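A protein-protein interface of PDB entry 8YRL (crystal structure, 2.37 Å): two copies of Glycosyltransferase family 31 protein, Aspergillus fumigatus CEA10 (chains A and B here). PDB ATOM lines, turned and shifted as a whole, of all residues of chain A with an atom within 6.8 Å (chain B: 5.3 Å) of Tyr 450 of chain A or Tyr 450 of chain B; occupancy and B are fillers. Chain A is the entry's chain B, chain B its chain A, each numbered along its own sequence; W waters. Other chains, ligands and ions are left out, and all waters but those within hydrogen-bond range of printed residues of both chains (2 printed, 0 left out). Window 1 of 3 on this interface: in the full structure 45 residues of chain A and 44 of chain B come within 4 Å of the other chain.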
ATOM      1  N   PRO A  43     -20.918 -35.361  12.851  1.00  0.00           N
ATOM      2  CA  PRO A  43     -20.879 -33.973  13.318  1.00  0.00           C
ATOM      3  C   PRO A  43     -22.278 -33.431  13.545  1.00  0.00           C
ATOM      4  O   PRO A  43     -23.194 -33.689  12.750  1.00  0.00           O
ATOM      5  CB  PRO A  43     -20.176 -33.237  12.169  1.00  0.00           C
ATOM      6  CG  PRO A  43     -20.509 -34.039  10.964  1.00  0.00           C
ATOM      7  CD  PRO A  43     -20.579 -35.474  11.421  1.00  0.00           C
ATOM      8  N   PRO A  44     -22.483 -32.677  14.625  1.00  0.00           N
ATOM      9  CA  PRO A  44     -23.780 -32.012  14.836  1.00  0.00           C
ATOM     10  C   PRO A  44     -23.937 -30.861  13.857  1.00  0.00           C
ATOM     11  O   PRO A  44     -23.108 -29.950  13.812  1.00  0.00           O
ATOM     12  CB  PRO A  44     -23.695 -31.516  16.287  1.00  0.00           C
ATOM     13  CG  PRO A  44     -22.493 -32.196  16.876  1.00  0.00           C
ATOM     14  CD  PRO A  44     -21.560 -32.446  15.744  1.00  0.00           C
ATOM     15  N   LEU A  45     -25.002 -30.904  13.068  1.00  0.00           N
ATOM     16  CA  LEU A  45     -25.210 -29.924  12.006  1.00  0.00           C
ATOM     17  C   LEU A  45     -26.516 -29.175  12.214  1.00  0.00           C
ATOM     18  O   LEU A  45     -27.600 -29.772  12.069  1.00  0.00           O
ATOM     19  CB  LEU A  45     -25.213 -30.607  10.638  1.00  0.00           C
ATOM     20  CG  LEU A  45     -23.957 -30.432   9.783  1.00  0.00           C
ATOM     21  CD1 LEU A  45     -22.720 -30.747  10.602  1.00  0.00           C
ATOM     22  CD2 LEU A  45     -24.025 -31.309   8.543  1.00  0.00           C
ATOM     23  N   PRO A  46     -26.477 -27.890  12.553  1.00  0.00           N
ATOM     24  CA  PRO A  46     -27.680 -27.067  12.423  1.00  0.00           C
ATOM     25  C   PRO A  46     -28.049 -26.921  10.956  1.00  0.00           C
ATOM     26  O   PRO A  46     -27.224 -27.110  10.059  1.00  0.00           O
ATOM     27  CB  PRO A  46     -27.264 -25.725  13.034  1.00  0.00           C
ATOM     28  CG  PRO A  46     -25.783 -25.677  12.831  1.00  0.00           C
ATOM     29  CD  PRO A  46     -25.310 -27.101  12.985  1.00  0.00           C
ATOM     30  N   PHE A  47     -29.318 -26.589  10.713  1.00  0.00           N
ATOM     31  CA  PHE A  47     -29.791 -26.502   9.337  1.00  0.00           C
ATOM     32  C   PHE A  47     -29.055 -25.434   8.538  1.00  0.00           C
ATOM     33  O   PHE A  47     -28.995 -25.530   7.307  1.00  0.00           O
ATOM     34  CB  PHE A  47     -31.298 -26.244   9.309  1.00  0.00           C
ATOM     35  CG  PHE A  47     -32.095 -27.382   8.737  1.00  0.00           C
ATOM     36  CD1 PHE A  47     -31.656 -28.689   8.874  1.00  0.00           C
ATOM     37  CD2 PHE A  47     -33.276 -27.145   8.053  1.00  0.00           C
ATOM     38  CE1 PHE A  47     -32.386 -29.739   8.348  1.00  0.00           C
ATOM     39  CE2 PHE A  47     -34.009 -28.191   7.524  1.00  0.00           C
ATOM     40  CZ  PHE A  47     -33.563 -29.489   7.671  1.00  0.00           C
ATOM     41  N   THR A  48     -28.483 -24.428   9.206  1.00  0.00           N
ATOM     42  CA  THR A  48     -27.672 -23.440   8.502  1.00  0.00           C
ATOM     43  C   THR A  48     -26.423 -24.069   7.896  1.00  0.00           C
ATOM     44  O   THR A  48     -25.887 -23.554   6.909  1.00  0.00           O
ATOM     45  CB  THR A  48     -27.285 -22.303   9.450  1.00  0.00           C
ATOM     46  OG1 THR A  48     -26.707 -22.846  10.643  1.00  0.00           O
ATOM     47  CG2 THR A  48     -28.508 -21.476   9.816  1.00  0.00           C
ATOM     48  N   GLU A  49     -25.945 -25.170   8.473  1.00  0.00           N
ATOM     49  CA  GLU A  49     -24.818 -25.911   7.922  1.00  0.00           C
ATOM     50  C   GLU A  49     -25.240 -27.182   7.202  1.00  0.00           C
ATOM     51  O   GLU A  49     -24.518 -27.646   6.313  1.00  0.00           O
ATOM     52  CB  GLU A  49     -23.826 -26.273   9.034  1.00  0.00           C
ATOM     53  CG  GLU A  49     -23.353 -25.088   9.861  1.00  0.00           C
ATOM     54  CD  GLU A  49     -22.661 -24.026   9.028  1.00  0.00           C
ATOM     55  OE1 GLU A  49     -21.945 -24.389   8.071  1.00  0.00           O
ATOM     56  OE2 GLU A  49     -22.838 -22.826   9.328  1.00  0.00           O
ATOM     57  N   LYS A 349     -18.757 -19.285  22.441  1.00  0.00           N
ATOM     58  CA  LYS A 349     -18.422 -20.302  21.450  1.00  0.00           C
ATOM     59  C   LYS A 349     -16.922 -20.551  21.392  1.00  0.00           C
ATOM     60  O   LYS A 349     -16.488 -21.677  21.121  1.00  0.00           O
ATOM     61  CB  LYS A 349     -18.937 -19.883  20.073  1.00  0.00           C
ATOM     62  CG  LYS A 349     -20.229 -20.555  19.644  1.00  0.00           C
ATOM     63  CD  LYS A 349     -20.556 -20.215  18.199  1.00  0.00           C
ATOM     64  CE  LYS A 349     -22.053 -20.083  17.981  1.00  0.00           C
ATOM     65  NZ  LYS A 349     -22.389 -19.918  16.539  1.00  0.00           N
ATOM     66  N   THR A 352     -15.689 -23.060  24.053  1.00  0.00           N
ATOM     67  CA  THR A 352     -16.365 -24.355  24.076  1.00  0.00           C
ATOM     68  C   THR A 352     -15.363 -25.504  24.135  1.00  0.00           C
ATOM     69  O   THR A 352     -15.611 -26.518  24.799  1.00  0.00           O
ATOM     70  CB  THR A 352     -17.267 -24.489  22.849  1.00  0.00           C
ATOM     71  OG1 THR A 352     -18.187 -23.390  22.808  1.00  0.00           O
ATOM     72  CG2 THR A 352     -18.049 -25.792  22.892  1.00  0.00           C
ATOM     73  N   ARG A 447     -17.432 -20.769  13.508  1.00  0.00           N
ATOM     74  CA  ARG A 447     -18.850 -20.505  13.299  1.00  0.00           C
ATOM     75  C   ARG A 447     -19.733 -21.210  14.322  1.00  0.00           C
ATOM     76  O   ARG A 447     -20.642 -20.594  14.884  1.00  0.00           O
ATOM     77  CB  ARG A 447     -19.255 -20.925  11.879  1.00  0.00           C
ATOM     78  CG  ARG A 447     -20.745 -20.833  11.593  1.00  0.00           C
ATOM     79  CD  ARG A 447     -21.151 -19.416  11.216  1.00  0.00           C
ATOM     80  NE  ARG A 447     -20.006 -18.614  10.803  1.00  0.00           N
ATOM     81  CZ  ARG A 447     -19.785 -18.202   9.562  1.00  0.00           C
ATOM     82  NH1 ARG A 447     -20.615 -18.501   8.575  1.00  0.00           N
ATOM     83  NH2 ARG A 447     -18.702 -17.474   9.303  1.00  0.00           N
ATOM     84  N   GLU A 448     -19.483 -22.493  14.576  1.00  0.00           N
ATOM     85  CA  GLU A 448     -20.270 -23.263  15.527  1.00  0.00           C
ATOM     86  C   GLU A 448     -19.344 -24.089  16.407  1.00  0.00           C
ATOM     87  O   GLU A 448     -18.216 -24.412  16.021  1.00  0.00           O
ATOM     88  CB  GLU A 448     -21.276 -24.186  14.822  1.00  0.00           C
ATOM     89  CG  GLU A 448     -22.208 -23.480  13.847  1.00  0.00           C
ATOM     90  CD  GLU A 448     -23.252 -22.627  14.543  1.00  0.00           C
ATOM     91  OE1 GLU A 448     -23.420 -22.768  15.773  1.00  0.00           O
ATOM     92  OE2 GLU A 448     -23.903 -21.809  13.859  1.00  0.00           O
ATOM     93  N   ALA A 449     -19.835 -24.430  17.596  1.00  0.00           N
ATOM     94  CA  ALA A 449     -19.081 -25.244  18.540  1.00  0.00           C
ATOM     95  C   ALA A 449     -20.059 -25.971  19.450  1.00  0.00           C
ATOM     96  O   ALA A 449     -20.970 -25.349  20.003  1.00  0.00           O
ATOM     97  CB  ALA A 449     -18.114 -24.388  19.363  1.00  0.00           C
ATOM     98  N   TYR A 450     -19.870 -27.281  19.602  1.00  0.00           N
ATOM     99  CA  TYR A 450     -20.790 -28.109  20.367  1.00  0.00           C
ATOM    100  C   TYR A 450     -20.018 -29.120  21.198  1.00  0.00           C
ATOM    101  O   TYR A 450     -18.963 -29.611  20.789  1.00  0.00           O
ATOM    102  CB  TYR A 450     -21.778 -28.845  19.451  1.00  0.00           C
ATOM    103  CG  TYR A 450     -22.461 -27.948  18.445  1.00  0.00           C
ATOM    104  CD1 TYR A 450     -23.368 -26.981  18.853  1.00  0.00           C
ATOM    105  CD2 TYR A 450     -22.193 -28.065  17.087  1.00  0.00           C
ATOM    106  CE1 TYR A 450     -23.990 -26.155  17.941  1.00  0.00           C
ATOM    107  CE2 TYR A 450     -22.814 -27.243  16.165  1.00  0.00           C
ATOM    108  CZ  TYR A 450     -23.712 -26.291  16.599  1.00  0.00           C
ATOM    109  OH  TYR A 450     -24.334 -25.470  15.688  1.00  0.00           O
ATOM    110  N   VAL A 451     -20.562 -29.428  22.371  1.00  0.00           N
ATOM    111  CA  VAL A 451     -20.031 -30.466  23.248  1.00  0.00           C
ATOM    112  C   VAL A 451     -20.931 -31.685  23.125  1.00  0.00           C
ATOM    113  O   VAL A 451     -22.113 -31.634  23.489  1.00  0.00           O
ATOM    114  CB  VAL A 451     -19.944 -29.986  24.704  1.00  0.00           C
ATOM    115  CG1 VAL A 451     -19.191 -31.000  25.553  1.00  0.00           C
ATOM    116  CG2 VAL A 451     -19.272 -28.629  24.774  1.00  0.00           C
ATOM    117  N   VAL A 452     -20.382 -32.779  22.609  1.00  0.00           N
ATOM    118  CA  VAL A 452     -21.112 -34.029  22.431  1.00  0.00           C
ATOM    119  C   VAL A 452     -20.413 -35.069  23.296  1.00  0.00           C
ATOM    120  O   VAL A 452     -19.408 -35.662  22.883  1.00  0.00           O
ATOM    121  CB  VAL A 452     -21.166 -34.467  20.964  1.00  0.00           C
ATOM    122  CG1 VAL A 452     -22.113 -35.647  20.799  1.00  0.00           C
ATOM    123  CG2 VAL A 452     -21.595 -33.308  20.090  1.00  0.00           C
ATOM    124  N   ASN A 455     -16.512 -35.142  23.743  1.00  0.00           N
ATOM    125  CA  ASN A 455     -15.899 -34.509  22.586  1.00  0.00           C
ATOM    126  C   ASN A 455     -16.487 -33.123  22.355  1.00  0.00           C
ATOM    127  O   ASN A 455     -17.629 -32.841  22.732  1.00  0.00           O
ATOM    128  CB  ASN A 455     -16.084 -35.363  21.326  1.00  0.00           C
ATOM    129  CG  ASN A 455     -15.566 -36.776  21.499  1.00  0.00           C
ATOM    130  OD1 ASN A 455     -14.549 -37.001  22.155  1.00  0.00           O
ATOM    131  ND2 ASN A 455     -16.259 -37.737  20.900  1.00  0.00           N
ATOM    132  N   VAL A 456     -15.690 -32.260  21.732  1.00  0.00           N
ATOM    133  CA  VAL A 456     -16.108 -30.918  21.349  1.00  0.00           C
ATOM    134  C   VAL A 456     -15.874 -30.758  19.854  1.00  0.00           C
ATOM    135  O   VAL A 456     -14.767 -31.010  19.363  1.00  0.00           O
ATOM    136  CB  VAL A 456     -15.354 -29.833  22.140  1.00  0.00           C
ATOM    137  CG1 VAL A 456     -15.647 -28.456  21.564  1.00  0.00           C
ATOM    138  CG2 VAL A 456     -15.738 -29.888  23.611  1.00  0.00           C
ATOM    139  N   HIS A 457     -16.915 -30.349  19.136  1.00  0.00           N
ATOM    140  CA  HIS A 457     -16.848 -30.139  17.695  1.00  0.00           C
ATOM    141  C   HIS A 457     -16.708 -28.649  17.418  1.00  0.00           C
ATOM    142  O   HIS A 457     -17.534 -27.852  17.872  1.00  0.00           O
ATOM    143  CB  HIS A 457     -18.091 -30.695  17.002  1.00  0.00           C
ATOM    144  CG  HIS A 457     -18.232 -32.181  17.113  1.00  0.00           C
ATOM    145  ND1 HIS A 457     -18.109 -33.022  16.028  1.00  0.00           N
ATOM    146  CD2 HIS A 457     -18.488 -32.975  18.178  1.00  0.00           C
ATOM    147  CE1 HIS A 457     -18.280 -34.270  16.421  1.00  0.00           C
ATOM    148  NE2 HIS A 457     -18.513 -34.270  17.721  1.00  0.00           N
ATOM    149  N   GLN A 458     -15.670 -28.276  16.675  1.00  0.00           N
ATOM    150  CA  GLN A 458     -15.433 -26.893  16.282  1.00  0.00           C
ATOM    151  C   GLN A 458     -15.684 -26.765  14.788  1.00  0.00           C
ATOM    152  O   GLN A 458     -15.062 -27.473  13.989  1.00  0.00           O
ATOM    153  CB  GLN A 458     -14.012 -26.457  16.632  1.00  0.00           C
ATOM    154  CG  GLN A 458     -13.759 -26.279  18.117  1.00  0.00           C
ATOM    155  CD  GLN A 458     -12.328 -25.878  18.420  1.00  0.00           C
ATOM    156  OE1 GLN A 458     -11.381 -26.452  17.881  1.00  0.00           O
ATOM    157  NE2 GLN A 458     -12.164 -24.886  19.285  1.00  0.00           N
ATOM    158  N   TRP A 459     -16.584 -25.861  14.414  1.00  0.00           N
ATOM    159  CA  TRP A 459     -17.026 -25.688  13.031  1.00  0.00           C
ATOM    160  C   TRP A 459     -16.475 -24.359  12.515  1.00  0.00           C
ATOM    161  O   TRP A 459     -17.105 -23.310  12.661  1.00  0.00           O
ATOM    162  CB  TRP A 459     -18.555 -25.736  12.952  1.00  0.00           C
ATOM    163  CG  TRP A 459     -19.112 -26.119  11.610  1.00  0.00           C
ATOM    164  CD1 TRP A 459     -19.644 -25.280  10.673  1.00  0.00           C
ATOM    165  CD2 TRP A 459     -19.210 -27.441  11.064  1.00  0.00           C
ATOM    166  NE1 TRP A 459     -20.060 -25.997   9.576  1.00  0.00           N
ATOM    167  CE2 TRP A 459     -19.805 -27.326   9.792  1.00  0.00           C
ATOM    168  CE3 TRP A 459     -18.849 -28.711  11.528  1.00  0.00           C
ATOM    169  CZ2 TRP A 459     -20.049 -28.431   8.978  1.00  0.00           C
ATOM    170  CZ3 TRP A 459     -19.090 -29.805  10.716  1.00  0.00           C
ATOM    171  CH2 TRP A 459     -19.679 -29.657   9.455  1.00  0.00           C
ATOM    172  N   PRO B  44     -26.128 -33.018  21.446  1.00  0.00           N
ATOM    173  CA  PRO B  44     -25.218 -31.916  21.110  1.00  0.00           C
ATOM    174  C   PRO B  44     -25.585 -30.671  21.902  1.00  0.00           C
ATOM    175  O   PRO B  44     -26.740 -30.241  21.908  1.00  0.00           O
ATOM    176  CB  PRO B  44     -25.437 -31.716  19.605  1.00  0.00           C
ATOM    177  CG  PRO B  44     -26.161 -32.952  19.151  1.00  0.00           C
ATOM    178  CD  PRO B  44     -26.989 -33.375  20.313  1.00  0.00           C
ATOM    179  N   LEU B  45     -24.594 -30.093  22.569  1.00  0.00           N
ATOM    180  CA  LEU B  45     -24.820 -28.998  23.509  1.00  0.00           C
ATOM    181  C   LEU B  45     -23.856 -27.853  23.241  1.00  0.00           C
ATOM    182  O   LEU B  45     -22.640 -28.006  23.475  1.00  0.00           O
ATOM    183  CB  LEU B  45     -24.666 -29.492  24.944  1.00  0.00           C
ATOM    184  CG  LEU B  45     -25.874 -30.185  25.565  1.00  0.00           C
ATOM    185  CD1 LEU B  45     -25.407 -31.356  26.394  1.00  0.00           C
ATOM    186  CD2 LEU B  45     -26.646 -29.210  26.426  1.00  0.00           C
ATOM    187  N   PRO B  46     -24.334 -26.710  22.758  1.00  0.00           N
ATOM    188  CA  PRO B  46     -23.501 -25.507  22.776  1.00  0.00           C
ATOM    189  C   PRO B  46     -23.271 -25.054  24.208  1.00  0.00           C
ATOM    190  O   PRO B  46     -24.006 -25.417  25.130  1.00  0.00           O
ATOM    191  CB  PRO B  46     -24.333 -24.487  21.992  1.00  0.00           C
ATOM    192  CG  PRO B  46     -25.742 -24.939  22.195  1.00  0.00           C
ATOM    193  CD  PRO B  46     -25.676 -26.445  22.213  1.00  0.00           C
ATOM    194  N   THR B 352     -35.824 -28.109  10.942  1.00  0.00           N
ATOM    195  CA  THR B 352     -34.697 -29.030  11.062  1.00  0.00           C
ATOM    196  C   THR B 352     -35.163 -30.477  11.173  1.00  0.00           C
ATOM    197  O   THR B 352     -34.487 -31.386  10.678  1.00  0.00           O
ATOM    198  CB  THR B 352     -33.842 -28.654  12.274  1.00  0.00           C
ATOM    199  OG1 THR B 352     -33.559 -27.249  12.246  1.00  0.00           O
ATOM    200  CG2 THR B 352     -32.535 -29.428  12.273  1.00  0.00           C
ATOM    201  N   GLU B 448     -32.901 -24.851  20.130  1.00  0.00           N
ATOM    202  CA  GLU B 448     -31.832 -25.355  19.283  1.00  0.00           C
ATOM    203  C   GLU B 448     -32.314 -26.599  18.551  1.00  0.00           C
ATOM    204  O   GLU B 448     -33.239 -27.288  18.994  1.00  0.00           O
ATOM    205  CB  GLU B 448     -30.566 -25.676  20.095  1.00  0.00           C
ATOM    206  CG  GLU B 448     -29.999 -24.505  20.893  1.00  0.00           C
ATOM    207  CD  GLU B 448     -29.392 -23.425  20.015  1.00  0.00           C
ATOM    208  OE1 GLU B 448     -29.150 -23.687  18.818  1.00  0.00           O
ATOM    209  OE2 GLU B 448     -29.155 -22.311  20.524  1.00  0.00           O
ATOM    210  N   ALA B 449     -31.673 -26.880  17.416  1.00  0.00           N
ATOM    211  CA  ALA B 449     -31.982 -28.065  16.629  1.00  0.00           C
ATOM    212  C   ALA B 449     -30.762 -28.428  15.799  1.00  0.00           C
ATOM    213  O   ALA B 449     -30.170 -27.556  15.155  1.00  0.00           O
ATOM    214  CB  ALA B 449     -33.200 -27.831  15.727  1.00  0.00           C
ATOM    215  N   TYR B 450     -30.388 -29.707  15.816  1.00  0.00           N
ATOM    216  CA  TYR B 450     -29.194 -30.176  15.126  1.00  0.00           C
ATOM    217  C   TYR B 450     -29.462 -31.525  14.478  1.00  0.00           C
ATOM    218  O   TYR B 450     -30.176 -32.362  15.039  1.00  0.00           O
ATOM    219  CB  TYR B 450     -28.002 -30.302  16.086  1.00  0.00           C
ATOM    220  CG  TYR B 450     -27.832 -29.121  17.007  1.00  0.00           C
ATOM    221  CD1 TYR B 450     -27.358 -27.908  16.529  1.00  0.00           C
ATOM    222  CD2 TYR B 450     -28.146 -29.216  18.356  1.00  0.00           C
ATOM    223  CE1 TYR B 450     -27.204 -26.824  17.365  1.00  0.00           C
ATOM    224  CE2 TYR B 450     -27.993 -28.136  19.203  1.00  0.00           C
ATOM    225  CZ  TYR B 450     -27.520 -26.941  18.700  1.00  0.00           C
ATOM    226  OH  TYR B 450     -27.364 -25.860  19.533  1.00  0.00           O
ATOM    227  N   VAL B 451     -28.880 -31.731  13.301  1.00  0.00           N
ATOM    228  CA  VAL B 451     -28.909 -33.016  12.614  1.00  0.00           C
ATOM    229  C   VAL B 451     -27.610 -33.743  12.930  1.00  0.00           C
ATOM    230  O   VAL B 451     -26.520 -33.250  12.615  1.00  0.00           O
ATOM    231  CB  VAL B 451     -29.092 -32.845  11.097  1.00  0.00           C
ATOM    232  CG1 VAL B 451     -29.421 -34.183  10.450  1.00  0.00           C
ATOM    233  CG2 VAL B 451     -30.179 -31.827  10.805  1.00  0.00           C
ATOM    234  N   VAL B 452     -27.722 -34.909  13.559  1.00  0.00           N
ATOM    235  CA  VAL B 452     -26.572 -35.732  13.925  1.00  0.00           C
ATOM    236  C   VAL B 452     -26.793 -37.098  13.290  1.00  0.00           C
ATOM    237  O   VAL B 452     -27.550 -37.923  13.816  1.00  0.00           O
ATOM    238  CB  VAL B 452     -26.395 -35.843  15.442  1.00  0.00           C
ATOM    239  CG1 VAL B 452     -25.105 -36.579  15.776  1.00  0.00           C
ATOM    240  CG2 VAL B 452     -26.403 -34.467  16.064  1.00  0.00           C
ATOM    241  N   ASN B 455     -30.347 -38.739  12.949  1.00  0.00           N
ATOM    242  CA  ASN B 455     -31.203 -38.240  14.013  1.00  0.00           C
ATOM    243  C   ASN B 455     -31.194 -36.718  14.048  1.00  0.00           C
ATOM    244  O   ASN B 455     -30.218 -36.072  13.655  1.00  0.00           O
ATOM    245  CB  ASN B 455     -30.764 -38.795  15.373  1.00  0.00           C
ATOM    246  CG  ASN B 455     -30.674 -40.310  15.384  1.00  0.00           C
ATOM    247  OD1 ASN B 455     -31.454 -40.994  14.722  1.00  0.00           O
ATOM    248  ND2 ASN B 455     -29.721 -40.840  16.143  1.00  0.00           N
ATOM    249  N   VAL B 456     -32.300 -36.152  14.525  1.00  0.00           N
ATOM    250  CA  VAL B 456     -32.452 -34.713  14.710  1.00  0.00           C
ATOM    251  C   VAL B 456     -32.757 -34.466  16.181  1.00  0.00           C
ATOM    252  O   VAL B 456     -33.712 -35.033  16.725  1.00  0.00           O
ATOM    253  CB  VAL B 456     -33.556 -34.131  13.814  1.00  0.00           C
ATOM    254  CG1 VAL B 456     -33.926 -32.728  14.272  1.00  0.00           C
ATOM    255  CG2 VAL B 456     -33.109 -34.119  12.361  1.00  0.00           C
ATOM    256  N   HIS B 457     -31.943 -33.632  16.822  1.00  0.00           N
ATOM    257  CA  HIS B 457     -32.121 -33.276  18.224  1.00  0.00           C
ATOM    258  C   HIS B 457     -32.840 -31.936  18.310  1.00  0.00           C
ATOM    259  O   HIS B 457     -32.307 -30.915  17.865  1.00  0.00           O
ATOM    260  CB  HIS B 457     -30.777 -33.199  18.944  1.00  0.00           C
ATOM    261  CG  HIS B 457     -30.039 -34.500  18.994  1.00  0.00           C
ATOM    262  ND1 HIS B 457     -29.810 -35.179  20.171  1.00  0.00           N
ATOM    263  CD2 HIS B 457     -29.475 -35.244  18.013  1.00  0.00           C
ATOM    264  CE1 HIS B 457     -29.138 -36.286  19.913  1.00  0.00           C
ATOM    265  NE2 HIS B 457     -28.924 -36.350  18.611  1.00  0.00           N
ATOM    266  N   GLN B 458     -34.040 -31.940  18.882  1.00  0.00           N
ATOM    267  CA  GLN B 458     -34.799 -30.719  19.112  1.00  0.00           C
ATOM    268  C   GLN B 458     -34.643 -30.300  20.569  1.00  0.00           C
ATOM    269  O   GLN B 458     -34.875 -31.104  21.477  1.00  0.00           O
ATOM    270  CB  GLN B 458     -36.277 -30.917  18.772  1.00  0.00           C
ATOM    271  CG  GLN B 458     -36.556 -31.091  17.290  1.00  0.00           C
ATOM    272  CD  GLN B 458     -38.030 -31.286  16.999  1.00  0.00           C
ATOM    273  OE1 GLN B 458     -38.723 -32.012  17.711  1.00  0.00           O
ATOM    274  NE2 GLN B 458     -38.516 -30.632  15.952  1.00  0.00           N
HETATM  275  O   HOH W   1     -30.898 -26.234  13.058  1.00  0.00           O
HETATM  276  O   HOH W   2     -26.160 -23.839  17.022  1.00  0.00           O
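Of the 20 printed residues of chain A, 8 touch a printed residue of chain B. Hydrophobic or aromatic side chains of chain A within 4 Å of the printed part of chain B: Pro 44, Leu 45, Phe 47, Tyr 450 and Val 451. Along chain B the printed residues that touch a printed residue of chain A span positions 44 to 452. Among the printed residues, 14 pairs touch across the chains. Among the printed residues, no Asp or Glu carboxylate lies within 4 Å of a Lys or Arg side-chain nitrogen of the other chain.
The backbone NH (N) of Val 451 of chain A sits at hydrogen-bond distance from the backbone carbonyl oxygen (O) of Leu 45 of chain B. The backbone carbonyl oxygen (O) of Leu 45 of chain A is in hydrogen-bond range of the backbone NH (N) of Val 451 of chain B (2.6 Å). The backbone carbonyl oxygen of Val 451 of chain B sits close to the backbone carbonyl oxygen of Pro 43 of chain A, 3.4 Å away.
CB of Pro 44 of chain A touches CB of Pro 44 of chain B (3.8 Å). C of Pro 44 of chain A touches O of Val 451 of chain B, 3.7 Å away. Val 452 of chain B touches Pro 44 of chain A. Leu 45 of chain A touches Tyr 450 of chain B (O to CA, 3.5 Å). Pro 46 of chain A touches Ala 449 of chain B. Phe 47 of chain A touches Thr 352 of chain B (CE1 to O, 3.5 Å). Val 451 of chain B touches Phe 47 of chain A (CG2 to CE1, 3.9 Å). CA of Pro 46 of chain B touches O of Ala 449 of chain A, 3.8 Å away. Tyr 450 of chain A touches Leu 45 of chain B (CA to O, 3.6 Å). Pro 44 of chain B touches Val 451 of chain A.
Water W1 lies within hydrogen-bond range of O of Ala 449 of chain B (2.6 Å), N of Phe 47 of chain A (2.8 Å) and OG1 of Thr 352 of chain B (3.0 Å). Water W2 lies within hydrogen-bond range of the side-chain hydroxyl of Tyr 450 of chain A (2.8 Å), the side-chain carboxylate of Glu 448 of chain A (3.2 Å), the side-chain hydroxyl of Tyr 450 of chain B (3.4 Å) and the side-chain carboxylate of Glu 448 of chain B (3.5 Å).
The side-chain hydroxyl of Tyr 450 of chain B lies within hydrogen-bond range of the side-chain carboxylate of Glu 448 of chain B, at 2.9 Å. O of Tyr 450 of chain B sits at hydrogen-bond distance from N of His 457 of chain B (2.8 Å). OE1 of Glu 448 of chain A sits at hydrogen-bond distance from OH of Tyr 450 of chain A (2.9 Å). N of His 457 of chain A is in hydrogen-bond range of O of Tyr 450 of chain A, 2.7 Å away.
Tyr 450 of chain A touches two residues of chain B. Printed residues of chain B within 4 Å of Val 451 of chain A: Pro 44 (3.9 Å) and Leu 45 (2.7 Å). Printed residues of chain A within 4 Å of Pro 46 of chain B: Ala 449 (3.8 Å). Tyr 450 of chain B touches just these residues of chain A: Leu 45 and Tyr 450. The nearest residue of chain B that does not touch Tyr 450 of chain A is Pro 46 of chain B (4.03 Å). The nearest residue of chain A that does not touch Tyr 450 of chain B is Pro 46 of chain A (4.1 Å). The nearest printed residue of chain B that does not touch Pro 43 of chain A is Val 452 of chain B (4.1 Å).
Pro 44 of chain B touches its own counterpart, Pro 44 of chain A. Pro 44 of chain A touches Val 452 of chain B, but with the chains exchanged Val 452 of chain A does not touch Pro 44 of chain B (4.01 Å). Pro 46 of chain A touches Ala 449 of chain B, and with the chains exchanged Ala 449 of chain A touches Pro 46 of chain B. Tyr 450 of chain A touches its own counterpart, Tyr 450 of chain B.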
